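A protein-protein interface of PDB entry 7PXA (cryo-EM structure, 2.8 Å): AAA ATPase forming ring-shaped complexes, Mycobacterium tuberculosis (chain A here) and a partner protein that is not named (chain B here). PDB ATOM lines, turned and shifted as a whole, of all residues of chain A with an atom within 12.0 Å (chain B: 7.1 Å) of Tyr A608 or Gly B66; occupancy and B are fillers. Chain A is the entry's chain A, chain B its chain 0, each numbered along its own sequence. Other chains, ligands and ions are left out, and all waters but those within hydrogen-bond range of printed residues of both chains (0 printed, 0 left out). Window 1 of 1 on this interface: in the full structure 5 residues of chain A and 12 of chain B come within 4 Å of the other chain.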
ATOM      1  N   LEU A 605     -24.004 -22.311  27.647  1.00  0.00           N
ATOM      2  CA  LEU A 605     -23.094 -22.378  28.786  1.00  0.00           C
ATOM      3  C   LEU A 605     -22.624 -20.994  29.216  1.00  0.00           C
ATOM      4  O   LEU A 605     -23.130 -19.983  28.724  1.00  0.00           O
ATOM      5  CB  LEU A 605     -21.887 -23.249  28.454  1.00  0.00           C
ATOM      6  CG  LEU A 605     -21.887 -24.650  29.055  1.00  0.00           C
ATOM      7  CD1 LEU A 605     -20.798 -25.488  28.417  1.00  0.00           C
ATOM      8  CD2 LEU A 605     -21.680 -24.569  30.554  1.00  0.00           C
ATOM      9  N   GLY A 606     -21.653 -20.954  30.120  1.00  0.00           N
ATOM     10  CA  GLY A 606     -21.164 -19.691  30.645  1.00  0.00           C
ATOM     11  C   GLY A 606     -19.752 -19.839  31.176  1.00  0.00           C
ATOM     12  O   GLY A 606     -19.148 -20.906  31.063  1.00  0.00           O
ATOM     13  N   GLN A 607     -19.221 -18.748  31.733  1.00  0.00           N
ATOM     14  CA  GLN A 607     -17.900 -18.749  32.369  1.00  0.00           C
ATOM     15  C   GLN A 607     -16.800 -19.087  31.358  1.00  0.00           C
ATOM     16  O   GLN A 607     -16.108 -20.100  31.479  1.00  0.00           O
ATOM     17  CB  GLN A 607     -17.868 -19.707  33.566  1.00  0.00           C
ATOM     18  CG  GLN A 607     -16.627 -19.602  34.434  1.00  0.00           C
ATOM     19  CD  GLN A 607     -16.688 -18.480  35.436  1.00  0.00           C
ATOM     20  OE1 GLN A 607     -17.357 -17.476  35.214  1.00  0.00           O
ATOM     21  NE2 GLN A 607     -15.999 -18.652  36.565  1.00  0.00           N
ATOM     22  N   TYR A 608     -16.668 -18.251  30.330  1.00  0.00           N
ATOM     23  CA  TYR A 608     -15.526 -18.307  29.423  1.00  0.00           C
ATOM     24  C   TYR A 608     -14.654 -17.073  29.632  1.00  0.00           C
ATOM     25  O   TYR A 608     -15.148 -15.949  29.618  1.00  0.00           O
ATOM     26  CB  TYR A 608     -15.983 -18.387  27.965  1.00  0.00           C
ATOM     27  CG  TYR A 608     -16.725 -19.660  27.650  1.00  0.00           C
ATOM     28  CD1 TYR A 608     -18.105 -19.727  27.773  1.00  0.00           C
ATOM     29  CD2 TYR A 608     -16.047 -20.800  27.241  1.00  0.00           C
ATOM     30  CE1 TYR A 608     -18.790 -20.890  27.496  1.00  0.00           C
ATOM     31  CE2 TYR A 608     -16.724 -21.968  26.961  1.00  0.00           C
ATOM     32  CZ  TYR A 608     -18.096 -22.008  27.090  1.00  0.00           C
ATOM     33  OH  TYR A 608     -18.774 -23.172  26.811  1.00  0.00           O
ATOM     34  N   LEU A 609     -13.355 -17.310  29.833  1.00  0.00           N
ATOM     35  CA  LEU A 609     -12.369 -16.251  30.019  1.00  0.00           C
ATOM     36  C   LEU A 609     -11.254 -16.409  28.987  1.00  0.00           C
ATOM     37  O   LEU A 609     -10.843 -15.456  28.328  1.00  0.00           O
ATOM     38  CB  LEU A 609     -11.794 -16.291  31.437  1.00  0.00           C
ATOM     39  CG  LEU A 609     -12.684 -15.797  32.577  1.00  0.00           C
ATOM     40  CD1 LEU A 609     -11.984 -15.990  33.911  1.00  0.00           C
ATOM     41  CD2 LEU A 609     -13.042 -14.334  32.360  1.00  0.00           C
ATOM     42  OXT LEU A 609     -10.747 -17.508  28.771  1.00  0.00           O
ATOM     43  N   LEU B  19     -16.805 -26.793  17.786  1.00  0.00           N
ATOM     44  CA  LEU B  19     -17.276 -26.427  19.118  1.00  0.00           C
ATOM     45  C   LEU B  19     -16.131 -25.912  19.978  1.00  0.00           C
ATOM     46  O   LEU B  19     -16.281 -24.914  20.695  1.00  0.00           O
ATOM     47  CB  LEU B  19     -17.955 -27.629  19.778  1.00  0.00           C
ATOM     48  CG  LEU B  19     -18.716 -27.424  21.091  1.00  0.00           C
ATOM     49  CD1 LEU B  19     -19.902 -28.373  21.159  1.00  0.00           C
ATOM     50  CD2 LEU B  19     -17.810 -27.630  22.296  1.00  0.00           C
ATOM     51  N   LYS B  22     -15.221 -22.421  18.745  1.00  0.00           N
ATOM     52  CA  LYS B  22     -16.221 -21.450  19.175  1.00  0.00           C
ATOM     53  C   LYS B  22     -16.066 -21.123  20.652  1.00  0.00           C
ATOM     54  O   LYS B  22     -16.189 -19.961  21.054  1.00  0.00           O
ATOM     55  CB  LYS B  22     -17.628 -21.977  18.888  1.00  0.00           C
ATOM     56  CG  LYS B  22     -17.983 -22.034  17.411  1.00  0.00           C
ATOM     57  CD  LYS B  22     -19.379 -22.599  17.202  1.00  0.00           C
ATOM     58  CE  LYS B  22     -19.716 -22.714  15.725  1.00  0.00           C
ATOM     59  NZ  LYS B  22     -18.767 -23.613  15.013  1.00  0.00           N
ATOM     60  N   GLY B  23     -15.798 -22.137  21.477  1.00  0.00           N
ATOM     61  CA  GLY B  23     -15.560 -21.882  22.889  1.00  0.00           C
ATOM     62  C   GLY B  23     -14.339 -21.017  23.128  1.00  0.00           C
ATOM     63  O   GLY B  23     -14.353 -20.130  23.985  1.00  0.00           O
ATOM     64  N   ILE B  24     -13.264 -21.264  22.375  1.00  0.00           N
ATOM     65  CA  ILE B  24     -12.048 -20.468  22.534  1.00  0.00           C
ATOM     66  C   ILE B  24     -12.286 -19.025  22.098  1.00  0.00           C
ATOM     67  O   ILE B  24     -11.892 -18.079  22.791  1.00  0.00           O
ATOM     68  CB  ILE B  24     -10.884 -21.110  21.758  1.00  0.00           C
ATOM     69  CG1 ILE B  24     -10.507 -22.455  22.380  1.00  0.00           C
ATOM     70  CG2 ILE B  24      -9.681 -20.180  21.733  1.00  0.00           C
ATOM     71  CD1 ILE B  24      -9.409 -23.182  21.639  1.00  0.00           C
ATOM     72  N   ALA B  25     -12.933 -18.833  20.945  1.00  0.00           N
ATOM     73  CA  ALA B  25     -13.159 -17.483  20.434  1.00  0.00           C
ATOM     74  C   ALA B  25     -14.150 -16.710  21.294  1.00  0.00           C
ATOM     75  O   ALA B  25     -14.176 -15.474  21.252  1.00  0.00           O
ATOM     76  CB  ALA B  25     -13.647 -17.544  18.987  1.00  0.00           C
ATOM     77  N   ARG B  26     -14.968 -17.412  22.074  1.00  0.00           N
ATOM     78  CA  ARG B  26     -15.939 -16.775  22.954  1.00  0.00           C
ATOM     79  C   ARG B  26     -15.286 -16.402  24.280  1.00  0.00           C
ATOM     80  O   ARG B  26     -15.796 -16.755  25.347  1.00  0.00           O
ATOM     81  CB  ARG B  26     -17.129 -17.712  23.179  1.00  0.00           C
ATOM     82  CG  ARG B  26     -18.396 -17.058  23.711  1.00  0.00           C
ATOM     83  CD  ARG B  26     -19.437 -18.119  24.042  1.00  0.00           C
ATOM     84  NE  ARG B  26     -20.661 -17.549  24.596  1.00  0.00           N
ATOM     85  CZ  ARG B  26     -21.677 -18.274  25.054  1.00  0.00           C
ATOM     86  NH1 ARG B  26     -21.617 -19.598  25.027  1.00  0.00           N
ATOM     87  NH2 ARG B  26     -22.756 -17.674  25.540  1.00  0.00           N
ATOM     88  N   ALA B  27     -14.163 -15.689  24.231  1.00  0.00           N
ATOM     89  CA  ALA B  27     -13.396 -15.397  25.436  1.00  0.00           C
ATOM     90  C   ALA B  27     -12.526 -14.170  25.186  1.00  0.00           C
ATOM     91  O   ALA B  27     -12.584 -13.546  24.124  1.00  0.00           O
ATOM     92  CB  ALA B  27     -12.557 -16.605  25.855  1.00  0.00           C
ATOM     93  N   LYS B  28     -11.713 -13.831  26.184  1.00  0.00           N
ATOM     94  CA  LYS B  28     -10.819 -12.685  26.117  1.00  0.00           C
ATOM     95  C   LYS B  28      -9.472 -13.091  25.525  1.00  0.00           C
ATOM     96  O   LYS B  28      -9.184 -14.270  25.315  1.00  0.00           O
ATOM     97  CB  LYS B  28     -10.631 -12.071  27.504  1.00  0.00           C
ATOM     98  CG  LYS B  28     -11.927 -11.677  28.191  1.00  0.00           C
ATOM     99  CD  LYS B  28     -12.674 -10.609  27.411  1.00  0.00           C
ATOM    100  CE  LYS B  28     -13.967 -10.224  28.111  1.00  0.00           C
ATOM    101  NZ  LYS B  28     -14.693  -9.154  27.376  1.00  0.00           N
ATOM    102  N   LYS B  52      -6.124 -15.515  34.831  1.00  0.00           N
ATOM    103  CA  LYS B  52      -5.756 -16.333  33.685  1.00  0.00           C
ATOM    104  C   LYS B  52      -4.256 -16.555  33.583  1.00  0.00           C
ATOM    105  O   LYS B  52      -3.809 -17.278  32.686  1.00  0.00           O
ATOM    106  CB  LYS B  52      -6.273 -15.689  32.394  1.00  0.00           C
ATOM    107  CG  LYS B  52      -7.724 -15.251  32.466  1.00  0.00           C
ATOM    108  CD  LYS B  52      -8.141 -14.510  31.207  1.00  0.00           C
ATOM    109  CE  LYS B  52      -8.020 -15.396  29.986  1.00  0.00           C
ATOM    110  NZ  LYS B  52      -8.461 -14.696  28.753  1.00  0.00           N
ATOM    111  N   ALA B  64      -3.592 -19.110  29.879  1.00  0.00           N
ATOM    112  CA  ALA B  64      -4.648 -19.908  29.275  1.00  0.00           C
ATOM    113  C   ALA B  64      -5.807 -19.006  28.878  1.00  0.00           C
ATOM    114  O   ALA B  64      -5.944 -17.882  29.366  1.00  0.00           O
ATOM    115  CB  ALA B  64      -5.129 -21.011  30.223  1.00  0.00           C
ATOM    116  N   ALA B  65      -6.641 -19.519  27.977  1.00  0.00           N
ATOM    117  CA  ALA B  65      -7.819 -18.799  27.511  1.00  0.00           C
ATOM    118  C   ALA B  65      -8.873 -19.810  27.089  1.00  0.00           C
ATOM    119  O   ALA B  65      -8.567 -20.760  26.362  1.00  0.00           O
ATOM    120  CB  ALA B  65      -7.476 -17.866  26.346  1.00  0.00           C
ATOM    121  N   GLY B  66     -10.094 -19.608  27.542  1.00  0.00           N
ATOM    122  CA  GLY B  66     -11.184 -20.501  27.221  1.00  0.00           C
ATOM    123  C   GLY B  66     -12.147 -20.604  28.398  1.00  0.00           C
ATOM    124  O   GLY B  66     -12.454 -19.604  29.049  1.00  0.00           O
ATOM    125  N   LYS B  67     -12.612 -21.824  28.650  1.00  0.00           N
ATOM    126  CA  LYS B  67     -13.549 -22.069  29.737  1.00  0.00           C
ATOM    127  C   LYS B  67     -12.781 -22.178  31.049  1.00  0.00           C
ATOM    128  O   LYS B  67     -11.870 -23.004  31.174  1.00  0.00           O
ATOM    129  CB  LYS B  67     -14.357 -23.334  29.469  1.00  0.00           C
ATOM    130  CG  LYS B  67     -15.720 -23.326  30.129  1.00  0.00           C
ATOM    131  CD  LYS B  67     -16.506 -24.578  29.799  1.00  0.00           C
ATOM    132  CE  LYS B  67     -17.939 -24.460  30.285  1.00  0.00           C
ATOM    133  NZ  LYS B  67     -18.017 -24.174  31.744  1.00  0.00           N
ATOM    134  N   PHE B  68     -13.158 -21.352  32.030  1.00  0.00           N
ATOM    135  CA  PHE B  68     -12.353 -21.212  33.241  1.00  0.00           C
ATOM    136  C   PHE B  68     -12.262 -22.518  34.019  1.00  0.00           C
ATOM    137  O   PHE B  68     -11.178 -22.902  34.476  1.00  0.00           O
ATOM    138  CB  PHE B  68     -12.919 -20.105  34.127  1.00  0.00           C
ATOM    139  CG  PHE B  68     -12.163 -19.915  35.410  1.00  0.00           C
ATOM    140  CD1 PHE B  68     -10.981 -19.194  35.431  1.00  0.00           C
ATOM    141  CD2 PHE B  68     -12.630 -20.461  36.594  1.00  0.00           C
ATOM    142  CE1 PHE B  68     -10.281 -19.020  36.608  1.00  0.00           C
ATOM    143  CE2 PHE B  68     -11.934 -20.291  37.774  1.00  0.00           C
ATOM    144  CZ  PHE B  68     -10.758 -19.569  37.781  1.00  0.00           C
ATOM    145  N   ASN B  69     -13.385 -23.221  34.178  1.00  0.00           N
ATOM    146  CA  ASN B  69     -13.397 -24.418  35.011  1.00  0.00           C
ATOM    147  C   ASN B  69     -12.567 -25.550  34.424  1.00  0.00           C
ATOM    148  O   ASN B  69     -12.315 -26.537  35.123  1.00  0.00           O
ATOM    149  CB  ASN B  69     -14.831 -24.898  35.235  1.00  0.00           C
ATOM    150  CG  ASN B  69     -15.476 -25.413  33.968  1.00  0.00           C
ATOM    151  OD1 ASN B  69     -15.293 -24.850  32.890  1.00  0.00           O
ATOM    152  ND2 ASN B  69     -16.233 -26.498  34.088  1.00  0.00           N
ATOM    153  N   GLU B  70     -12.140 -25.436  33.168  1.00  0.00           N
ATOM    154  CA  GLU B  70     -11.317 -26.462  32.541  1.00  0.00           C
ATOM    155  C   GLU B  70      -9.828 -26.148  32.656  1.00  0.00           C
ATOM    156  O   GLU B  70      -9.050 -26.980  33.138  1.00  0.00           O
ATOM    157  CB  GLU B  70     -11.723 -26.626  31.074  1.00  0.00           C
ATOM    158  CG  GLU B  70     -13.173 -27.040  30.888  1.00  0.00           C
ATOM    159  CD  GLU B  70     -13.601 -27.038  29.436  1.00  0.00           C
ATOM    160  OE1 GLU B  70     -12.816 -26.573  28.584  1.00  0.00           O
ATOM    161  OE2 GLU B  70     -14.724 -27.503  29.146  1.00  0.00           O
ATOM    162  N   PHE B  71      -9.408 -24.954  32.230  1.00  0.00           N
ATOM    163  CA  PHE B  71      -7.988 -24.649  32.329  1.00  0.00           C
ATOM    164  C   PHE B  71      -7.555 -24.362  33.759  1.00  0.00           C
ATOM    165  O   PHE B  71      -6.373 -24.510  34.064  1.00  0.00           O
ATOM    166  CB  PHE B  71      -7.593 -23.495  31.392  1.00  0.00           C
ATOM    167  CG  PHE B  71      -8.183 -22.152  31.742  1.00  0.00           C
ATOM    168  CD1 PHE B  71      -7.690 -21.405  32.800  1.00  0.00           C
ATOM    169  CD2 PHE B  71      -9.181 -21.602  30.957  1.00  0.00           C
ATOM    170  CE1 PHE B  71      -8.216 -20.164  33.100  1.00  0.00           C
ATOM    171  CE2 PHE B  71      -9.707 -20.358  31.248  1.00  0.00           C
ATOM    172  CZ  PHE B  71      -9.225 -19.639  32.323  1.00  0.00           C
ATOM    173  N   LYS B 116     -17.196 -34.062  25.667  1.00  0.00           N
ATOM    174  CA  LYS B 116     -16.971 -32.715  25.182  1.00  0.00           C
ATOM    175  C   LYS B 116     -15.497 -32.359  25.310  1.00  0.00           C
ATOM    176  O   LYS B 116     -14.923 -32.497  26.401  1.00  0.00           O
ATOM    177  CB  LYS B 116     -17.822 -31.698  25.960  1.00  0.00           C
ATOM    178  CG  LYS B 116     -17.741 -30.280  25.414  1.00  0.00           C
ATOM    179  CD  LYS B 116     -18.523 -29.305  26.279  1.00  0.00           C
ATOM    180  CE  LYS B 116     -17.908 -29.178  27.662  1.00  0.00           C
ATOM    181  NZ  LYS B 116     -16.513 -28.661  27.599  1.00  0.00           N
ATOM    182  N   GLU B 119     -12.477 -26.682  25.816  1.00  0.00           N
ATOM    183  CA  GLU B 119     -12.476 -25.488  24.973  1.00  0.00           C
ATOM    184  C   GLU B 119     -11.493 -24.452  25.520  1.00  0.00           C
ATOM    185  O   GLU B 119     -11.845 -23.321  25.849  1.00  0.00           O
ATOM    186  CB  GLU B 119     -13.887 -24.925  24.873  1.00  0.00           C
ATOM    187  CG  GLU B 119     -14.944 -25.995  24.642  1.00  0.00           C
ATOM    188  CD  GLU B 119     -16.348 -25.508  24.922  1.00  0.00           C
ATOM    189  OE1 GLU B 119     -16.653 -24.342  24.602  1.00  0.00           O
ATOM    190  OE2 GLU B 119     -17.149 -26.293  25.471  1.00  0.00           O
ATOM    191  N   VAL B 120     -10.228 -24.868  25.610  1.00  0.00           N
ATOM    192  CA  VAL B 120      -9.177 -24.060  26.210  1.00  0.00           C
ATOM    193  C   VAL B 120      -7.971 -24.025  25.282  1.00  0.00           C
ATOM    194  O   VAL B 120      -7.809 -24.864  24.395  1.00  0.00           O
ATOM    195  CB  VAL B 120      -8.758 -24.586  27.600  1.00  0.00           C
ATOM    196  CG1 VAL B 120      -9.918 -24.495  28.577  1.00  0.00           C
ATOM    197  CG2 VAL B 120      -8.255 -26.015  27.494  1.00  0.00           C
ATOM    198  N   GLU B 121      -7.120 -23.023  25.502  1.00  0.00           N
ATOM    199  CA  GLU B 121      -5.871 -22.868  24.765  1.00  0.00           C
ATOM    200  C   GLU B 121      -4.787 -22.479  25.757  1.00  0.00           C
ATOM    201  O   GLU B 121      -4.857 -21.404  26.361  1.00  0.00           O
ATOM    202  CB  GLU B 121      -6.011 -21.814  23.663  1.00  0.00           C
ATOM    203  CG  GLU B 121      -4.779 -21.634  22.797  1.00  0.00           C
ATOM    204  CD  GLU B 121      -5.027 -20.696  21.631  1.00  0.00           C
ATOM    205  OE1 GLU B 121      -6.207 -20.451  21.304  1.00  0.00           O
ATOM    206  OE2 GLU B 121      -4.045 -20.200  21.044  1.00  0.00           O
ATOM    207  N   GLY B 157      -6.959 -16.661  22.550  1.00  0.00           N
ATOM    208  CA  GLY B 157      -8.268 -16.152  22.913  1.00  0.00           C
ATOM    209  C   GLY B 157      -8.776 -15.027  22.035  1.00  0.00           C
ATOM    210  O   GLY B 157      -7.998 -14.185  21.577  1.00  0.00           O
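Printed residues of chain B that touch a printed residue of chain A: Gly B23, Arg B26, Ala B27, Lys B28, Lys B52, Ala B65, Gly B66, Lys B67, Phe B68, Phe B71 and Glu B119.
Hydrophobic or aromatic side chains of chain B within 4 Å of the printed part of chain A: Ala B27, Phe B68 and Phe B71.
Of the 5 printed residues of chain A, 5 touch a printed residue of chain B.
Hydrophobic or aromatic side chains of chain A that line the printed part of chain B: Leu A605, Tyr A608 and Leu A609.
Among the printed residues, 17 pairs touch across the chains.
Among the printed residues, no Asp or Glu carboxylate lies within 4 Å of a Lys or Arg side-chain nitrogen of the other chain.
The backbone NH (N) of Lys B28 is in hydrogen-bond range of the chain-end carboxylate (O) of Leu A609 (2.8 Å).
NZ of Lys B52 lies within salt-bridge range of O of Leu A609 (2.5 Å).
N of Gly B66 sits at hydrogen-bond distance from OXT of Leu A609 (2.5 Å).
N of Phe B68 sits at hydrogen-bond distance from O of Gln A607, 3.3 Å away.
The side-chain hydroxyl (OH) of Tyr A608 is in hydrogen-bond range of the side-chain carboxylate (OE1) of Glu B119, at 3.3 Å.
CE of Lys B67 touches CD1 of Leu A605, at 3.6 Å.
Gly A606 touches Lys B67 (O to NZ, 3.5 Å).
CG of Lys B67 touches O of Gln A607, at 3.5 Å.
Tyr A608 touches Arg B26 (CB to O, 3.1 Å).
Tyr A608 touches Gly B66 (CA to O, 3.4 Å).
Tyr A608 touches Lys B67.
Leu A609 touches Ala B27.
Leu A609 touches Ala B65.
CD1 of Leu A609 touches CD1 of Phe B68 (3.7 Å).
Leu A609 touches Phe B71.
The backbone carbonyl oxygen of Lys B52 is in hydrogen-bond range of the backbone NH of Ala B64 (3.4 Å).
N of Glu B121 is in hydrogen-bond range of O of Ala B65 (2.8 Å).
The side-chain amino group (NZ) of Lys B67 lies within hydrogen-bond range of the side-chain amide oxygen (OD1) of Asn B69, at 3.0 Å.
The backbone carbonyl oxygen (O) of Glu B119 sits at hydrogen-bond distance from the backbone NH (N) of Lys B67.
The side-chain carboxylate (OE1) of Glu B70 is in hydrogen-bond range of the backbone NH (N) of Glu B119, at 2.8 Å.
The side-chain carboxylate of Glu B119 is in salt-bridge range of the side-chain amino group of Lys B116, 3.2 Å away.
Printed residues of chain B within 4 Å of Tyr A608: Gly B23 (3.7 Å), Arg B26 (3.1 Å), Gly B66 (3.4 Å), Lys B67 (3.6 Å) and Glu B119 (3.3 Å).
Of chain A, only Tyr A608 (3.4 Å) and Leu A609 (2.5 Å) come within 4 Å of Gly B66.
Gly B23 touches one residue of chain A.
Ile B24 touches none of the printed residues of chain A.
Lys B28 touches just one residue of chain A: Leu A609 (2.8 Å).
No residue of chain A comes within 4 Å of Ala B64.
Of chain A, only Leu A609 comes within 4 Å of Ala B65.
Of the printed residues of chain B, Gln A607 touches Lys B67 (3.5 Å) and Phe B68 (3.3 Å).
Of the printed residues of chain A, Lys B52 touches Leu A609 (2.5 Å).
The nearest residue of chain A that does not touch Gly B66 is Gln A607 (4.4 Å).
The nearest printed residue of chain A that does not touch Phe B68 is Tyr A608 (4.7 Å).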
